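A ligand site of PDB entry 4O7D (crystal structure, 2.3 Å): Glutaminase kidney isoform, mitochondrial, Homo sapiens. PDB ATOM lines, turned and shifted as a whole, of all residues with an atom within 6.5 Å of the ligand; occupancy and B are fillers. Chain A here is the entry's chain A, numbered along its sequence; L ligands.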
ATOM      1  N   TYR A  31      -7.275  25.586 -16.800  1.00  0.00           N
ATOM      2  CA  TYR A  31      -7.159  26.734 -15.914  1.00  0.00           C
ATOM      3  C   TYR A  31      -5.685  27.141 -15.740  1.00  0.00           C
ATOM      4  O   TYR A  31      -5.397  28.304 -15.431  1.00  0.00           O
ATOM      5  CB  TYR A  31      -7.890  26.539 -14.569  1.00  0.00           C
ATOM      6  CG  TYR A  31      -7.255  25.533 -13.632  1.00  0.00           C
ATOM      7  CD1 TYR A  31      -6.312  25.929 -12.702  1.00  0.00           C
ATOM      8  CD2 TYR A  31      -7.598  24.184 -13.681  1.00  0.00           C
ATOM      9  CE1 TYR A  31      -5.714  25.018 -11.848  1.00  0.00           C
ATOM     10  CE2 TYR A  31      -7.006  23.271 -12.820  1.00  0.00           C
ATOM     11  CZ  TYR A  31      -6.064  23.688 -11.910  1.00  0.00           C
ATOM     12  OH  TYR A  31      -5.459  22.780 -11.063  1.00  0.00           O
ATOM     13  N   LEU A  66      -0.782  14.149  -9.837  1.00  0.00           N
ATOM     14  CA  LEU A  66      -1.812  13.548  -9.000  1.00  0.00           C
ATOM     15  C   LEU A  66      -2.979  14.523  -8.856  1.00  0.00           C
ATOM     16  O   LEU A  66      -4.130  14.139  -9.024  1.00  0.00           O
ATOM     17  CB  LEU A  66      -1.250  13.197  -7.620  1.00  0.00           C
ATOM     18  CG  LEU A  66      -0.455  11.890  -7.619  1.00  0.00           C
ATOM     19  CD1 LEU A  66       0.323  11.726  -6.325  1.00  0.00           C
ATOM     20  CD2 LEU A  66      -1.369  10.710  -7.898  1.00  0.00           C
ATOM     21  N   GLN A  67      -2.679  15.776  -8.560  1.00  0.00           N
ATOM     22  CA  GLN A  67      -3.721  16.762  -8.284  1.00  0.00           C
ATOM     23  C   GLN A  67      -4.617  16.203  -7.174  1.00  0.00           C
ATOM     24  O   GLN A  67      -4.109  15.735  -6.162  1.00  0.00           O
ATOM     25  CB  GLN A  67      -4.490  17.088  -9.554  1.00  0.00           C
ATOM     26  CG  GLN A  67      -3.681  17.890 -10.573  1.00  0.00           C
ATOM     27  CD  GLN A  67      -3.523  19.332 -10.171  1.00  0.00           C
ATOM     28  OE1 GLN A  67      -4.066  19.757  -9.146  1.00  0.00           O
ATOM     29  NE2 GLN A  67      -2.771  20.096 -10.949  1.00  0.00           N
ATOM     30  N   SER A  68      -5.945  16.222  -7.331  1.00  0.00           N
ATOM     31  CA  SER A  68      -6.755  15.801  -6.193  1.00  0.00           C
ATOM     32  C   SER A  68      -6.581  14.312  -5.896  1.00  0.00           C
ATOM     33  O   SER A  68      -6.965  13.835  -4.826  1.00  0.00           O
ATOM     34  CB  SER A  68      -8.228  16.172  -6.369  1.00  0.00           C
ATOM     35  OG  SER A  68      -8.434  17.536  -6.016  1.00  0.00           O
ATOM     36  N   CYS A  69      -5.979  13.566  -6.815  1.00  0.00           N
ATOM     37  CA  CYS A  69      -5.719  12.152  -6.540  1.00  0.00           C
ATOM     38  C   CYS A  69      -4.832  11.976  -5.307  1.00  0.00           C
ATOM     39  O   CYS A  69      -4.789  10.901  -4.731  1.00  0.00           O
ATOM     40  CB  CYS A  69      -5.085  11.446  -7.749  1.00  0.00           C
ATOM     41  SG  CYS A  69      -6.203  11.339  -9.166  1.00  0.00           S
ATOM     42  N   LYS A  71      -5.216  13.563  -2.462  1.00  0.00           N
ATOM     43  CA  LYS A  71      -5.962  13.876  -1.243  1.00  0.00           C
ATOM     44  C   LYS A  71      -6.105  12.650  -0.332  1.00  0.00           C
ATOM     45  O   LYS A  71      -5.773  12.710   0.834  1.00  0.00           O
ATOM     46  CB  LYS A  71      -7.324  14.494  -1.566  1.00  0.00           C
ATOM     47  CG  LYS A  71      -7.247  15.970  -1.961  1.00  0.00           C
ATOM     48  CD  LYS A  71      -8.539  16.441  -2.607  1.00  0.00           C
ATOM     49  CE  LYS A  71      -8.631  17.963  -2.636  1.00  0.00           C
ATOM     50  NZ  LYS A  71      -7.589  18.611  -3.487  1.00  0.00           N
ATOM     51  N   PHE A 100     -19.521  20.199  -4.673  1.00  0.00           N
ATOM     52  CA  PHE A 100     -18.153  19.985  -4.215  1.00  0.00           C
ATOM     53  C   PHE A 100     -17.363  21.305  -4.164  1.00  0.00           C
ATOM     54  O   PHE A 100     -17.399  22.115  -5.105  1.00  0.00           O
ATOM     55  CB  PHE A 100     -17.451  18.965  -5.127  1.00  0.00           C
ATOM     56  CG  PHE A 100     -16.700  17.879  -4.393  1.00  0.00           C
ATOM     57  CD1 PHE A 100     -15.294  17.820  -4.458  1.00  0.00           C
ATOM     58  CD2 PHE A 100     -17.394  16.935  -3.641  1.00  0.00           C
ATOM     59  CE1 PHE A 100     -14.582  16.817  -3.785  1.00  0.00           C
ATOM     60  CE2 PHE A 100     -16.702  15.924  -2.946  1.00  0.00           C
ATOM     61  CZ  PHE A 100     -15.289  15.868  -3.018  1.00  0.00           C
ATOM     62  N   ASN A 101     -16.667  21.521  -3.046  1.00  0.00           N
ATOM     63  CA  ASN A 101     -15.859  22.738  -2.849  1.00  0.00           C
ATOM     64  C   ASN A 101     -16.629  24.048  -3.063  1.00  0.00           C
ATOM     65  O   ASN A 101     -16.230  24.866  -3.901  1.00  0.00           O
ATOM     66  CB  ASN A 101     -14.580  22.716  -3.709  1.00  0.00           C
ATOM     67  CG  ASN A 101     -13.710  21.484  -3.462  1.00  0.00           C
ATOM     68  OD1 ASN A 101     -12.994  21.412  -2.469  1.00  0.00           O
ATOM     69  ND2 ASN A 101     -13.772  20.516  -4.374  1.00  0.00           N
ATOM     70  N   MET A 115     -11.580  14.931   1.244  1.00  0.00           N
ATOM     71  CA  MET A 115     -11.543  14.876  -0.215  1.00  0.00           C
ATOM     72  C   MET A 115     -11.975  16.163  -0.897  1.00  0.00           C
ATOM     73  O   MET A 115     -12.006  16.225  -2.126  1.00  0.00           O
ATOM     74  CB  MET A 115     -12.416  13.718  -0.728  1.00  0.00           C
ATOM     75  CG  MET A 115     -12.099  12.390  -0.107  1.00  0.00           C
ATOM     76  SD  MET A 115     -10.336  12.015  -0.172  1.00  0.00           S
ATOM     77  CE  MET A 115     -10.237  10.544   0.841  1.00  0.00           C
ATOM     78  N   ASN A 117     -11.281  20.490  -1.063  1.00  0.00           N
ATOM     79  CA  ASN A 117     -10.092  21.325  -0.910  1.00  0.00           C
ATOM     80  C   ASN A 117      -9.899  21.838   0.530  1.00  0.00           C
ATOM     81  O   ASN A 117      -8.812  21.699   1.108  1.00  0.00           O
ATOM     82  CB  ASN A 117     -10.120  22.501  -1.895  1.00  0.00           C
ATOM     83  CG  ASN A 117      -9.905  22.063  -3.343  1.00  0.00           C
ATOM     84  OD1 ASN A 117      -9.856  20.864  -3.668  1.00  0.00           O
ATOM     85  ND2 ASN A 117      -9.811  23.036  -4.221  1.00  0.00           N
ATOM     86  N   GLU A 163      -0.027  26.797 -10.074  1.00  0.00           N
ATOM     87  CA  GLU A 163      -1.097  26.540  -9.096  1.00  0.00           C
ATOM     88  C   GLU A 163      -1.103  27.662  -8.066  1.00  0.00           C
ATOM     89  O   GLU A 163      -2.146  28.221  -7.761  1.00  0.00           O
ATOM     90  CB  GLU A 163      -0.927  25.189  -8.393  1.00  0.00           C
ATOM     91  CG  GLU A 163      -1.195  23.963  -9.277  1.00  0.00           C
ATOM     92  CD  GLU A 163      -2.682  23.614  -9.401  1.00  0.00           C
ATOM     93  OE1 GLU A 163      -3.021  22.767 -10.255  1.00  0.00           O
ATOM     94  OE2 GLU A 163      -3.502  24.168  -8.621  1.00  0.00           O
ATOM     95  N   ASN A 170      -8.223  28.893  -3.557  1.00  0.00           N
ATOM     96  CA  ASN A 170      -7.567  28.189  -2.453  1.00  0.00           C
ATOM     97  C   ASN A 170      -7.039  29.165  -1.411  1.00  0.00           C
ATOM     98  O   ASN A 170      -6.952  28.826  -0.230  1.00  0.00           O
ATOM     99  CB  ASN A 170      -6.459  27.276  -2.949  1.00  0.00           C
ATOM    100  CG  ASN A 170      -6.991  26.056  -3.677  1.00  0.00           C
ATOM    101  OD1 ASN A 170      -7.881  25.367  -3.192  1.00  0.00           O
ATOM    102  ND2 ASN A 170      -6.457  25.792  -4.862  1.00  0.00           N
ATOM    103  N   TYR A 196       0.508  22.600   0.052  1.00  0.00           N
ATOM    104  CA  TYR A 196      -0.645  22.014  -0.593  1.00  0.00           C
ATOM    105  C   TYR A 196      -0.491  22.046  -2.125  1.00  0.00           C
ATOM    106  O   TYR A 196      -0.723  21.041  -2.800  1.00  0.00           O
ATOM    107  CB  TYR A 196      -1.923  22.750  -0.160  1.00  0.00           C
ATOM    108  CG  TYR A 196      -3.157  22.394  -0.976  1.00  0.00           C
ATOM    109  CD1 TYR A 196      -3.907  21.249  -0.693  1.00  0.00           C
ATOM    110  CD2 TYR A 196      -3.572  23.206  -2.020  1.00  0.00           C
ATOM    111  CE1 TYR A 196      -5.046  20.927  -1.440  1.00  0.00           C
ATOM    112  CE2 TYR A 196      -4.698  22.888  -2.782  1.00  0.00           C
ATOM    113  CZ  TYR A 196      -5.432  21.760  -2.492  1.00  0.00           C
ATOM    114  OH  TYR A 196      -6.548  21.457  -3.254  1.00  0.00           O
ATOM    115  N   PHE A 197      -0.107  23.191  -2.667  1.00  0.00           N
ATOM    116  CA  PHE A 197       0.149  23.300  -4.108  1.00  0.00           C
ATOM    117  C   PHE A 197       1.219  22.329  -4.576  1.00  0.00           C
ATOM    118  O   PHE A 197       1.105  21.740  -5.636  1.00  0.00           O
ATOM    119  CB  PHE A 197       0.598  24.708  -4.457  1.00  0.00           C
ATOM    120  CG  PHE A 197      -0.437  25.739  -4.174  1.00  0.00           C
ATOM    121  CD1 PHE A 197      -0.100  26.911  -3.512  1.00  0.00           C
ATOM    122  CD2 PHE A 197      -1.749  25.536  -4.575  1.00  0.00           C
ATOM    123  CE1 PHE A 197      -1.071  27.869  -3.252  1.00  0.00           C
ATOM    124  CE2 PHE A 197      -2.720  26.495  -4.316  1.00  0.00           C
ATOM    125  CZ  PHE A 197      -2.366  27.662  -3.655  1.00  0.00           C
ATOM    126  N   CYS A 200      -0.162  18.784  -4.818  1.00  0.00           N
ATOM    127  CA  CYS A 200      -0.996  18.616  -6.002  1.00  0.00           C
ATOM    128  C   CYS A 200      -0.114  18.405  -7.202  1.00  0.00           C
ATOM    129  O   CYS A 200      -0.538  17.785  -8.178  1.00  0.00           O
ATOM    130  CB  CYS A 200      -1.860  19.851  -6.243  1.00  0.00           C
ATOM    131  SG  CYS A 200      -3.152  20.113  -5.003  1.00  0.00           S
ATOM    132  N   TYR A 248     -15.994  13.937  -6.711  1.00  0.00           N
ATOM    133  CA  TYR A 248     -16.663  15.226  -6.744  1.00  0.00           C
ATOM    134  C   TYR A 248     -18.181  15.041  -6.616  1.00  0.00           C
ATOM    135  O   TYR A 248     -18.640  14.172  -5.876  1.00  0.00           O
ATOM    136  CB  TYR A 248     -16.337  15.975  -8.048  1.00  0.00           C
ATOM    137  CG  TYR A 248     -14.849  16.112  -8.360  1.00  0.00           C
ATOM    138  CD1 TYR A 248     -13.997  16.850  -7.541  1.00  0.00           C
ATOM    139  CD2 TYR A 248     -14.304  15.531  -9.494  1.00  0.00           C
ATOM    140  CE1 TYR A 248     -12.648  16.978  -7.828  1.00  0.00           C
ATOM    141  CE2 TYR A 248     -12.963  15.657  -9.801  1.00  0.00           C
ATOM    142  CZ  TYR A 248     -12.137  16.385  -8.983  1.00  0.00           C
ATOM    143  OH  TYR A 248     -10.789  16.493  -9.305  1.00  0.00           O
ATOM    144  N   LYS A 263     -10.742   7.896  -6.511  1.00  0.00           N
ATOM    145  CA  LYS A 263     -10.505   9.332  -6.388  1.00  0.00           C
ATOM    146  C   LYS A 263     -10.054   9.882  -7.706  1.00  0.00           C
ATOM    147  O   LYS A 263      -8.992   9.506  -8.206  1.00  0.00           O
ATOM    148  CB  LYS A 263      -9.442   9.630  -5.327  1.00  0.00           C
ATOM    149  CG  LYS A 263      -9.183  11.115  -5.140  1.00  0.00           C
ATOM    150  CD  LYS A 263     -10.250  11.768  -4.281  1.00  0.00           C
ATOM    151  CE  LYS A 263     -10.292  13.271  -4.496  1.00  0.00           C
ATOM    152  NZ  LYS A 263     -11.103  13.633  -5.694  1.00  0.00           N
ATOM    153  N   SER A 264     -10.852  10.777  -8.272  1.00  0.00           N
ATOM    154  CA  SER A 264     -10.474  11.447  -9.502  1.00  0.00           C
ATOM    155  C   SER A 264      -9.638  12.716  -9.248  1.00  0.00           C
ATOM    156  O   SER A 264      -9.535  13.193  -8.125  1.00  0.00           O
ATOM    157  CB  SER A 264     -11.715  11.749 -10.329  1.00  0.00           C
ATOM    158  OG  SER A 264     -12.471  12.756  -9.692  1.00  0.00           O
ATOM    159  N   GLY A 265      -9.014  13.237 -10.309  1.00  0.00           N
ATOM    160  CA  GLY A 265      -8.246  14.475 -10.251  1.00  0.00           C
ATOM    161  C   GLY A 265      -8.341  15.220 -11.574  1.00  0.00           C
ATOM    162  O   GLY A 265      -8.691  14.640 -12.607  1.00  0.00           O
ATOM    163  N   VAL A 266      -8.045  16.510 -11.546  1.00  0.00           N
ATOM    164  CA  VAL A 266      -8.290  17.366 -12.700  1.00  0.00           C
ATOM    165  C   VAL A 266      -7.319  17.080 -13.875  1.00  0.00           C
ATOM    166  O   VAL A 266      -7.562  17.521 -14.994  1.00  0.00           O
ATOM    167  CB  VAL A 266      -8.263  18.877 -12.280  1.00  0.00           C
ATOM    168  CG1 VAL A 266      -6.832  19.342 -12.040  1.00  0.00           C
ATOM    169  CG2 VAL A 266      -8.979  19.750 -13.309  1.00  0.00           C
ATOM    170  N   ALA A 267      -6.238  16.340 -13.625  1.00  0.00           N
ATOM    171  CA  ALA A 267      -5.312  15.918 -14.681  1.00  0.00           C
ATOM    172  C   ALA A 267      -5.886  14.769 -15.463  1.00  0.00           C
ATOM    173  O   ALA A 267      -5.326  14.361 -16.468  1.00  0.00           O
ATOM    174  CB  ALA A 267      -3.952  15.505 -14.093  1.00  0.00           C
HETATM  175  N1  LIG L   1      -5.208  21.992  -7.934  1.00  0.00           N
HETATM  176  C1  LIG L   1      -6.667  21.835  -8.091  1.00  0.00           C
HETATM  177  C2  LIG L   1      -7.366  22.572  -6.901  1.00  0.00           C
HETATM  178  O1  LIG L   1      -8.510  23.095  -7.076  1.00  0.00           O
HETATM  179  O2  LIG L   1      -6.706  22.616  -5.835  1.00  0.00           O
HETATM  180  C3  LIG L   1      -7.042  20.347  -8.162  1.00  0.00           C
HETATM  181  C4  LIG L   1      -8.516  19.997  -8.442  1.00  0.00           C
HETATM  182  C5  LIG L   1      -8.554  18.479  -8.360  1.00  0.00           C
HETATM  183  O3  LIG L   1      -7.819  17.774  -9.034  1.00  0.00           O
HETATM  184  C6  LIG L   1      -9.256  17.892  -7.114  1.00  0.00           C
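The side-chain hydroxyl (OG) of Ser 68 lies within hydrogen-bond range of the side-chain amino group (NZ) of Lys 71 (2.9 Å).
The side-chain amide oxygen (OD1) of Asn 117 lies within hydrogen-bond range of the side-chain hydroxyl (OH) of Tyr 196 (3.4 Å).
SG of Cys 200 sits at hydrogen-bond distance from O of Tyr 196, at 3.4 Å.
The side-chain hydroxyl of Tyr 196 sits at hydrogen-bond distance from the side-chain amino group of Lys 71, at 3.0 Å.
The side-chain carboxylate (OE1) of Glu 163 is in hydrogen-bond range of the side-chain hydroxyl (OH) of Tyr 31 (2.6 Å).
The side-chain amide oxygen (OD1) of Asn 117 is in hydrogen-bond range of the side-chain amino group (NZ) of Lys 71.
The backbone NH (N) of Asn 117 lies within hydrogen-bond range of the side-chain amide oxygen (OD1) of Asn 101 (2.4 Å).
SG of Cys 69 lies within hydrogen-bond range of N of Gly 265 (3.6 Å).
N of Ser 68 sits at hydrogen-bond distance from O3 of the ligand (3.0 Å).
The side-chain hydroxyl (OG) of Ser 68 is bonded to a carbon (C6) of the ligand.
The side-chain amide oxygen of Gln 67 is in hydrogen-bond range of a nitrogen (N1) of the ligand (2.8 Å).
N of Val 266 lies within hydrogen-bond range of O3 of the ligand (2.8 Å).
An oxygen (O2) of the ligand is in hydrogen-bond range of the side-chain hydroxyl of Tyr 196 (2.8 Å).
The side-chain carboxylate of Glu 163 lies within salt-bridge range of a nitrogen (N1) of the ligand (2.8 Å).
The side-chain hydroxyl of Tyr 248 sits close to an oxygen (O3) of the ligand (3.2 Å).
The side-chain amide nitrogen of Asn 117 lies within hydrogen-bond range of an oxygen (O1) of the ligand, at 3.1 Å.
The side-chain hydroxyl of Tyr 31 sits at hydrogen-bond distance from a nitrogen (N1) of the ligand (3.2 Å).
ND2 of Asn 170 sits at hydrogen-bond distance from O2 of the ligand, 3.3 Å away.
Residues that only touch the ligand: Gly 265 (3.5 Å).
Hydrophobic or aromatic side chains that line the ligand: Tyr 196, Tyr 248 and Val 266.
Of the 21 residues printed, 10 come within 4 Å of the ligand.
The nearest printed residue that does not touch the ligand is Cys 200 (4.04 Å).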
